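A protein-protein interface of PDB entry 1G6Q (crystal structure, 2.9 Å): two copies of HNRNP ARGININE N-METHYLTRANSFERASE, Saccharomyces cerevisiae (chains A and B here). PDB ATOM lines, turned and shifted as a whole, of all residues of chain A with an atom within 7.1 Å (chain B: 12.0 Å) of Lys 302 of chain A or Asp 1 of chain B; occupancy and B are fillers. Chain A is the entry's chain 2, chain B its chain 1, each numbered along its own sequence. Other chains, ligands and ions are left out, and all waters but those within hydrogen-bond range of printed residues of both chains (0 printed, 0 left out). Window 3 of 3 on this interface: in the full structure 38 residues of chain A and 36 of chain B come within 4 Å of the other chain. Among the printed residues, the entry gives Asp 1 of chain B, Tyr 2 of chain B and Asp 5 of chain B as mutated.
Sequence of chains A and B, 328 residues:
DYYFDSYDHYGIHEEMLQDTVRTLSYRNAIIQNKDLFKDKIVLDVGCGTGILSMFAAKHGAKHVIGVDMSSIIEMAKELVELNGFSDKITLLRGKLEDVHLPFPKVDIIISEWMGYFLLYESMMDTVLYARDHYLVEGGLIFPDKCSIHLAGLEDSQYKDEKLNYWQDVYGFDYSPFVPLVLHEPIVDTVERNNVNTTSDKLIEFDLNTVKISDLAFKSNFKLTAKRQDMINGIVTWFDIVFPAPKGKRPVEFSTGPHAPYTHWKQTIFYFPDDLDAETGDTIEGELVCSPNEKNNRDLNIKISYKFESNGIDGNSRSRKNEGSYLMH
OD2 of Asp 1 of chain B lies within hydrogen-bond range of OG of Ser 324 of chain A, 3.2 Å away. OE2 of Glu 322 of chain A lies close to OD2 of Asp 1 of chain B, at 3.0 Å. OD1 of Asp 1 of chain B lies within salt-bridge range of NZ of Lys 302 of chain A (3.0 Å).
Printed residues of chain A that touch a printed residue of chain B: Asn 300, Lys 302, Glu 322, Ser 324 and Tyr 325. Hydrophobic or aromatic side chains of chain B that line the printed part of chain A: Phe 4. Along chain B the printed residues that touch a printed residue of chain A span positions 1 to 4. Among the printed residues, Asp or Glu carboxylates within 4 Å of a Lys or Arg side-chain nitrogen of the other chain: Lys 302 of chain A with Asp 1 of chain B (3.0 Å).
No position is printed for both chains.
Lys 302 of chain A touches just one residue of chain B: Asp 1. Of chain A, only Lys 302, Glu 322 and Ser 324 come within 4 Å of Asp 1 of chain B. No residue of chain B comes within 4 Å of Glu 286 of chain A. No residue of chain B comes within 4 Å of Leu 287 of chain A. Val 288 of chain A touches none of the printed residues of chain B. No residue of chain B comes within 4 Å of Cys 289 of chain A. No residue of chain B comes within 4 Å of Ile 301 of chain A. No residue of chain B comes within 4 Å of Ile 303 of chain A. No residue of chain B comes within 4 Å of Ser 304 of chain A. Gly 323 of chain A touches none of the printed residues of chain B. Tyr 325 of chain A touches just one residue of chain B: Phe 4. Of the printed residues of chain A, Phe 4 of chain B touches Asn 300 (3.3 Å), Ser 324 (3.5 Å) and Tyr 325 (3.8 Å). Of the printed residues of chain B, Asn 300 of chain A touches Phe 4 (3.3 Å). Of the printed residues of chain A, Tyr 2 of chain B touches Ser 324. Tyr 3 of chain B touches none of the printed residues of chain A. The nearest residue of chain A that does not touch Asp 1 of chain B is Gly 323 of chain A (5.1 Å). The nearest printed residue of chain A that does not touch Tyr 2 of chain B is Asn 300 of chain A (5.0 Å).
The backbone carbonyl oxygen (O) of Ile 301 of chain A sits at hydrogen-bond distance from the backbone NH (N) of Tyr 325 of chain A (2.8 Å). The backbone NH (N) of Asn 300 of chain A sits at hydrogen-bond distance from the backbone carbonyl oxygen (O) of Ser 290 of chain A (2.9 Å). NZ of Lys 302 of chain A is in salt-bridge range of OE1 of Glu 322 of chain A (3.6 Å). The backbone NH (N) of Lys 302 of chain A sits at hydrogen-bond distance from the backbone carbonyl oxygen (O) of Val 288 of chain A.
Asn 300 of chain A touches Phe 4 of chain B (ND2 to CD2, 3.3 Å). Ser 324 of chain A touches Tyr 2 of chain B (OG to N, 3.6 Å). Phe 4 of chain B touches Ser 324 of chain A. Phe 4 of chain B touches Tyr 325 of chain A (CE2 to C, 3.8 Å).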
ATOM      1  N   PHE A 221      16.427 -17.218 -20.483  1.00  0.00           N
ATOM      2  CA  PHE A 221      15.081 -17.663 -20.799  1.00  0.00           C
ATOM      3  C   PHE A 221      14.540 -17.165 -22.123  1.00  0.00           C
ATOM      4  O   PHE A 221      14.899 -16.086 -22.608  1.00  0.00           O
ATOM      5  CB  PHE A 221      14.098 -17.233 -19.691  1.00  0.00           C
ATOM      6  CG  PHE A 221      13.782 -15.747 -19.559  1.00  0.00           C
ATOM      7  CD1 PHE A 221      14.557 -14.944 -18.736  1.00  0.00           C
ATOM      8  CD2 PHE A 221      12.760 -15.185 -20.301  1.00  0.00           C
ATOM      9  CE1 PHE A 221      14.322 -13.570 -18.657  1.00  0.00           C
ATOM     10  CE2 PHE A 221      12.522 -13.811 -20.231  1.00  0.00           C
ATOM     11  CZ  PHE A 221      13.300 -12.998 -19.411  1.00  0.00           C
ATOM     12  N   PHE A 269       6.646  -9.095 -12.013  1.00  0.00           N
ATOM     13  CA  PHE A 269       7.681  -8.083 -12.213  1.00  0.00           C
ATOM     14  C   PHE A 269       7.346  -7.244 -13.445  1.00  0.00           C
ATOM     15  O   PHE A 269       7.143  -7.754 -14.553  1.00  0.00           O
ATOM     16  CB  PHE A 269       9.042  -8.639 -12.491  1.00  0.00           C
ATOM     17  CG  PHE A 269       9.558  -9.490 -11.364  1.00  0.00           C
ATOM     18  CD1 PHE A 269      10.376  -8.899 -10.411  1.00  0.00           C
ATOM     19  CD2 PHE A 269       9.242 -10.842 -11.330  1.00  0.00           C
ATOM     20  CE1 PHE A 269      10.892  -9.683  -9.402  1.00  0.00           C
ATOM     21  CE2 PHE A 269       9.754 -11.619 -10.319  1.00  0.00           C
ATOM     22  CZ  PHE A 269      10.582 -11.044  -9.355  1.00  0.00           C
ATOM     23  N   GLU A 286      17.355 -12.689 -19.512  1.00  0.00           N
ATOM     24  CA  GLU A 286      18.106 -13.267 -18.434  1.00  0.00           C
ATOM     25  C   GLU A 286      17.595 -12.761 -17.103  1.00  0.00           C
ATOM     26  O   GLU A 286      17.312 -11.570 -16.985  1.00  0.00           O
ATOM     27  CB  GLU A 286      19.561 -12.877 -18.650  1.00  0.00           C
ATOM     28  CG  GLU A 286      20.588 -13.058 -17.515  1.00  0.00           C
ATOM     29  CD  GLU A 286      22.017 -12.599 -17.847  1.00  0.00           C
ATOM     30  OE1 GLU A 286      22.388 -11.460 -17.546  1.00  0.00           O
ATOM     31  OE2 GLU A 286      22.775 -13.394 -18.399  1.00  0.00           O
ATOM     32  N   LEU A 287      17.463 -13.606 -16.090  1.00  0.00           N
ATOM     33  CA  LEU A 287      17.096 -13.135 -14.759  1.00  0.00           C
ATOM     34  C   LEU A 287      18.155 -13.534 -13.762  1.00  0.00           C
ATOM     35  O   LEU A 287      18.609 -14.664 -13.746  1.00  0.00           O
ATOM     36  CB  LEU A 287      15.749 -13.727 -14.325  1.00  0.00           C
ATOM     37  CG  LEU A 287      14.980 -13.201 -13.080  1.00  0.00           C
ATOM     38  CD1 LEU A 287      13.476 -13.444 -13.256  1.00  0.00           C
ATOM     39  CD2 LEU A 287      15.514 -13.873 -11.816  1.00  0.00           C
ATOM     40  N   VAL A 288      18.577 -12.628 -12.927  1.00  0.00           N
ATOM     41  CA  VAL A 288      19.530 -12.984 -11.919  1.00  0.00           C
ATOM     42  C   VAL A 288      18.869 -12.759 -10.588  1.00  0.00           C
ATOM     43  O   VAL A 288      18.101 -11.803 -10.404  1.00  0.00           O
ATOM     44  CB  VAL A 288      20.835 -12.130 -12.034  1.00  0.00           C
ATOM     45  CG1 VAL A 288      21.148 -11.920 -13.504  1.00  0.00           C
ATOM     46  CG2 VAL A 288      20.716 -10.774 -11.392  1.00  0.00           C
ATOM     47  N   CYS A 289      19.124 -13.627  -9.642  1.00  0.00           N
ATOM     48  CA  CYS A 289      18.528 -13.476  -8.342  1.00  0.00           C
ATOM     49  C   CYS A 289      19.606 -13.689  -7.335  1.00  0.00           C
ATOM     50  O   CYS A 289      20.298 -14.704  -7.380  1.00  0.00           O
ATOM     51  CB  CYS A 289      17.466 -14.492  -8.114  1.00  0.00           C
ATOM     52  SG  CYS A 289      16.756 -14.165  -6.504  1.00  0.00           S
ATOM     53  N   SER A 290      19.801 -12.710  -6.463  1.00  0.00           N
ATOM     54  CA  SER A 290      20.839 -12.799  -5.432  1.00  0.00           C
ATOM     55  C   SER A 290      20.442 -12.159  -4.111  1.00  0.00           C
ATOM     56  O   SER A 290      19.744 -11.129  -4.092  1.00  0.00           O
ATOM     57  CB  SER A 290      22.128 -12.108  -5.842  1.00  0.00           C
ATOM     58  OG  SER A 290      22.044 -10.688  -5.900  1.00  0.00           O
ATOM     59  N   ASN A 300      17.770  -9.045  -4.337  1.00  0.00           N
ATOM     60  CA  ASN A 300      18.024  -8.215  -5.506  1.00  0.00           C
ATOM     61  C   ASN A 300      17.765  -9.065  -6.722  1.00  0.00           C
ATOM     62  O   ASN A 300      18.417 -10.092  -6.873  1.00  0.00           O
ATOM     63  CB  ASN A 300      19.463  -7.776  -5.596  1.00  0.00           C
ATOM     64  CG  ASN A 300      19.627  -6.384  -5.040  1.00  0.00           C
ATOM     65  OD1 ASN A 300      19.511  -6.183  -3.844  1.00  0.00           O
ATOM     66  ND2 ASN A 300      19.836  -5.312  -5.783  1.00  0.00           N
ATOM     67  N   ILE A 301      16.817  -8.658  -7.561  1.00  0.00           N
ATOM     68  CA  ILE A 301      16.406  -9.329  -8.806  1.00  0.00           C
ATOM     69  C   ILE A 301      16.800  -8.434  -9.976  1.00  0.00           C
ATOM     70  O   ILE A 301      16.626  -7.203  -9.930  1.00  0.00           O
ATOM     71  CB  ILE A 301      14.868  -9.499  -8.979  1.00  0.00           C
ATOM     72  CG1 ILE A 301      14.142 -10.002  -7.752  1.00  0.00           C
ATOM     73  CG2 ILE A 301      14.663 -10.430 -10.133  1.00  0.00           C
ATOM     74  CD1 ILE A 301      14.316 -11.446  -7.287  1.00  0.00           C
ATOM     75  N   LYS A 302      17.331  -8.957 -11.061  1.00  0.00           N
ATOM     76  CA  LYS A 302      17.512  -8.092 -12.217  1.00  0.00           C
ATOM     77  C   LYS A 302      16.982  -8.803 -13.431  1.00  0.00           C
ATOM     78  O   LYS A 302      17.264  -9.986 -13.608  1.00  0.00           O
ATOM     79  CB  LYS A 302      18.961  -7.779 -12.480  1.00  0.00           C
ATOM     80  CG  LYS A 302      19.206  -6.848 -13.658  1.00  0.00           C
ATOM     81  CD  LYS A 302      20.655  -7.091 -13.973  1.00  0.00           C
ATOM     82  CE  LYS A 302      21.089  -6.573 -15.327  1.00  0.00           C
ATOM     83  NZ  LYS A 302      22.548  -6.672 -15.511  1.00  0.00           N
ATOM     84  N   ILE A 303      16.165  -8.154 -14.253  1.00  0.00           N
ATOM     85  CA  ILE A 303      15.661  -8.775 -15.471  1.00  0.00           C
ATOM     86  C   ILE A 303      16.107  -8.113 -16.758  1.00  0.00           C
ATOM     87  O   ILE A 303      15.803  -6.951 -17.017  1.00  0.00           O
ATOM     88  CB  ILE A 303      14.156  -8.791 -15.421  1.00  0.00           C
ATOM     89  CG1 ILE A 303      13.736  -9.664 -14.267  1.00  0.00           C
ATOM     90  CG2 ILE A 303      13.614  -9.298 -16.744  1.00  0.00           C
ATOM     91  CD1 ILE A 303      12.280  -9.562 -13.817  1.00  0.00           C
ATOM     92  N   SER A 304      16.820  -8.794 -17.608  1.00  0.00           N
ATOM     93  CA  SER A 304      17.250  -8.185 -18.850  1.00  0.00           C
ATOM     94  C   SER A 304      16.438  -8.804 -19.951  1.00  0.00           C
ATOM     95  O   SER A 304      16.279 -10.036 -19.942  1.00  0.00           O
ATOM     96  CB  SER A 304      18.681  -8.475 -19.179  1.00  0.00           C
ATOM     97  OG  SER A 304      19.554  -7.677 -18.395  1.00  0.00           O
ATOM     98  N   GLU A 322      16.622  -3.425 -19.490  1.00  0.00           N
ATOM     99  CA  GLU A 322      16.827  -4.223 -18.306  1.00  0.00           C
ATOM    100  C   GLU A 322      16.161  -3.582 -17.118  1.00  0.00           C
ATOM    101  O   GLU A 322      15.841  -2.398 -17.153  1.00  0.00           O
ATOM    102  CB  GLU A 322      18.313  -4.412 -18.000  1.00  0.00           C
ATOM    103  CG  GLU A 322      19.250  -3.206 -18.016  1.00  0.00           C
ATOM    104  CD  GLU A 322      20.641  -3.497 -17.466  1.00  0.00           C
ATOM    105  OE1 GLU A 322      21.279  -4.429 -17.959  1.00  0.00           O
ATOM    106  OE2 GLU A 322      21.070  -2.793 -16.546  1.00  0.00           O
ATOM    107  N   GLY A 323      15.894  -4.322 -16.058  1.00  0.00           N
ATOM    108  CA  GLY A 323      15.348  -3.732 -14.859  1.00  0.00           C
ATOM    109  C   GLY A 323      15.912  -4.347 -13.586  1.00  0.00           C
ATOM    110  O   GLY A 323      16.295  -5.523 -13.501  1.00  0.00           O
ATOM    111  N   SER A 324      15.973  -3.538 -12.554  1.00  0.00           N
ATOM    112  CA  SER A 324      16.423  -4.083 -11.302  1.00  0.00           C
ATOM    113  C   SER A 324      15.244  -3.909 -10.374  1.00  0.00           C
ATOM    114  O   SER A 324      14.542  -2.898 -10.373  1.00  0.00           O
ATOM    115  CB  SER A 324      17.615  -3.305 -10.869  1.00  0.00           C
ATOM    116  OG  SER A 324      18.509  -3.159 -11.974  1.00  0.00           O
ATOM    117  N   TYR A 325      14.954  -4.979  -9.662  1.00  0.00           N
ATOM    118  CA  TYR A 325      13.859  -5.048  -8.709  1.00  0.00           C
ATOM    119  C   TYR A 325      14.388  -5.409  -7.328  1.00  0.00           C
ATOM    120  O   TYR A 325      15.350  -6.167  -7.178  1.00  0.00           O
ATOM    121  CB  TYR A 325      12.864  -6.103  -9.156  1.00  0.00           C
ATOM    122  CG  TYR A 325      12.477  -5.965 -10.632  1.00  0.00           C
ATOM    123  CD1 TYR A 325      13.329  -6.492 -11.585  1.00  0.00           C
ATOM    124  CD2 TYR A 325      11.286  -5.348 -11.033  1.00  0.00           C
ATOM    125  CE1 TYR A 325      13.020  -6.407 -12.916  1.00  0.00           C
ATOM    126  CE2 TYR A 325      10.968  -5.262 -12.389  1.00  0.00           C
ATOM    127  CZ  TYR A 325      11.847  -5.792 -13.322  1.00  0.00           C
ATOM    128  OH  TYR A 325      11.627  -5.682 -14.669  1.00  0.00           O
ATOM    129  N   ASP B   1      23.487  -0.927 -13.713  1.00  0.00           N
ATOM    130  CA  ASP B   1      22.373  -1.256 -12.826  1.00  0.00           C
ATOM    131  C   ASP B   1      21.974  -0.322 -11.687  1.00  0.00           C
ATOM    132  O   ASP B   1      22.798   0.396 -11.101  1.00  0.00           O
ATOM    133  CB  ASP B   1      22.598  -2.637 -12.212  1.00  0.00           C
ATOM    134  CG  ASP B   1      22.248  -3.760 -13.174  1.00  0.00           C
ATOM    135  OD1 ASP B   1      23.093  -4.632 -13.386  1.00  0.00           O
ATOM    136  OD2 ASP B   1      21.128  -3.756 -13.699  1.00  0.00           O
ATOM    137  N   TYR B   2      20.672  -0.345 -11.371  1.00  0.00           N
ATOM    138  CA  TYR B   2      20.149   0.485 -10.286  1.00  0.00           C
ATOM    139  C   TYR B   2      20.438  -0.072  -8.874  1.00  0.00           C
ATOM    140  O   TYR B   2      19.966  -1.138  -8.455  1.00  0.00           O
ATOM    141  CB  TYR B   2      18.617   0.682 -10.458  1.00  0.00           C
ATOM    142  CG  TYR B   2      18.034   1.871  -9.667  1.00  0.00           C
ATOM    143  CD1 TYR B   2      17.878   3.107 -10.320  1.00  0.00           C
ATOM    144  CD2 TYR B   2      17.699   1.758  -8.297  1.00  0.00           C
ATOM    145  CE1 TYR B   2      17.406   4.219  -9.611  1.00  0.00           C
ATOM    146  CE2 TYR B   2      17.233   2.867  -7.586  1.00  0.00           C
ATOM    147  CZ  TYR B   2      17.094   4.098  -8.251  1.00  0.00           C
ATOM    148  OH  TYR B   2      16.701   5.238  -7.558  1.00  0.00           O
ATOM    149  N   TYR B   3      21.259   0.650  -8.115  1.00  0.00           N
ATOM    150  CA  TYR B   3      21.589   0.268  -6.738  1.00  0.00           C
ATOM    151  C   TYR B   3      20.523   0.552  -5.681  1.00  0.00           C
ATOM    152  O   TYR B   3      20.049   1.675  -5.454  1.00  0.00           O
ATOM    153  CB  TYR B   3      22.863   0.965  -6.290  1.00  0.00           C
ATOM    154  CG  TYR B   3      23.423   0.514  -4.943  1.00  0.00           C
ATOM    155  CD1 TYR B   3      23.923  -0.784  -4.796  1.00  0.00           C
ATOM    156  CD2 TYR B   3      23.480   1.414  -3.875  1.00  0.00           C
ATOM    157  CE1 TYR B   3      24.490  -1.188  -3.588  1.00  0.00           C
ATOM    158  CE2 TYR B   3      24.046   1.015  -2.661  1.00  0.00           C
ATOM    159  CZ  TYR B   3      24.554  -0.287  -2.521  1.00  0.00           C
ATOM    160  OH  TYR B   3      25.135  -0.686  -1.321  1.00  0.00           O
ATOM    161  N   PHE B   4      20.197  -0.504  -4.961  1.00  0.00           N
ATOM    162  CA  PHE B   4      19.177  -0.378  -3.945  1.00  0.00           C
ATOM    163  C   PHE B   4      19.576   0.131  -2.553  1.00  0.00           C
ATOM    164  O   PHE B   4      19.943  -0.564  -1.603  1.00  0.00           O
ATOM    165  CB  PHE B   4      18.497  -1.727  -3.889  1.00  0.00           C
ATOM    166  CG  PHE B   4      17.557  -1.831  -5.070  1.00  0.00           C
ATOM    167  CD1 PHE B   4      16.380  -1.054  -5.076  1.00  0.00           C
ATOM    168  CD2 PHE B   4      17.877  -2.654  -6.155  1.00  0.00           C
ATOM    169  CE1 PHE B   4      15.520  -1.098  -6.177  1.00  0.00           C
ATOM    170  CE2 PHE B   4      17.014  -2.687  -7.249  1.00  0.00           C
ATOM    171  CZ  PHE B   4      15.853  -1.915  -7.250  1.00  0.00           C
ATOM    172  N   ASP B   5      19.510   1.451  -2.482  1.00  0.00           N
ATOM    173  CA  ASP B   5      19.811   2.182  -1.251  1.00  0.00           C
ATOM    174  C   ASP B   5      18.602   2.545  -0.362  1.00  0.00           C
ATOM    175  O   ASP B   5      18.723   3.129   0.716  1.00  0.00           O
ATOM    176  CB  ASP B   5      20.604   3.473  -1.651  1.00  0.00           C
ATOM    177  CG  ASP B   5      19.903   4.518  -2.533  1.00  0.00           C
ATOM    178  OD1 ASP B   5      19.705   5.637  -2.068  1.00  0.00           O
ATOM    179  OD2 ASP B   5      19.573   4.233  -3.687  1.00  0.00           O
ATOM    180  N   SER B   6      17.384   2.202  -0.779  1.00  0.00           N
ATOM    181  CA  SER B   6      16.139   2.643  -0.123  1.00  0.00           C
ATOM    182  C   SER B   6      15.101   1.616   0.355  1.00  0.00           C
ATOM    183  O   SER B   6      14.847   0.627  -0.336  1.00  0.00           O
ATOM    184  CB  SER B   6      15.438   3.619  -1.075  1.00  0.00           C
ATOM    185  OG  SER B   6      15.263   3.082  -2.396  1.00  0.00           O
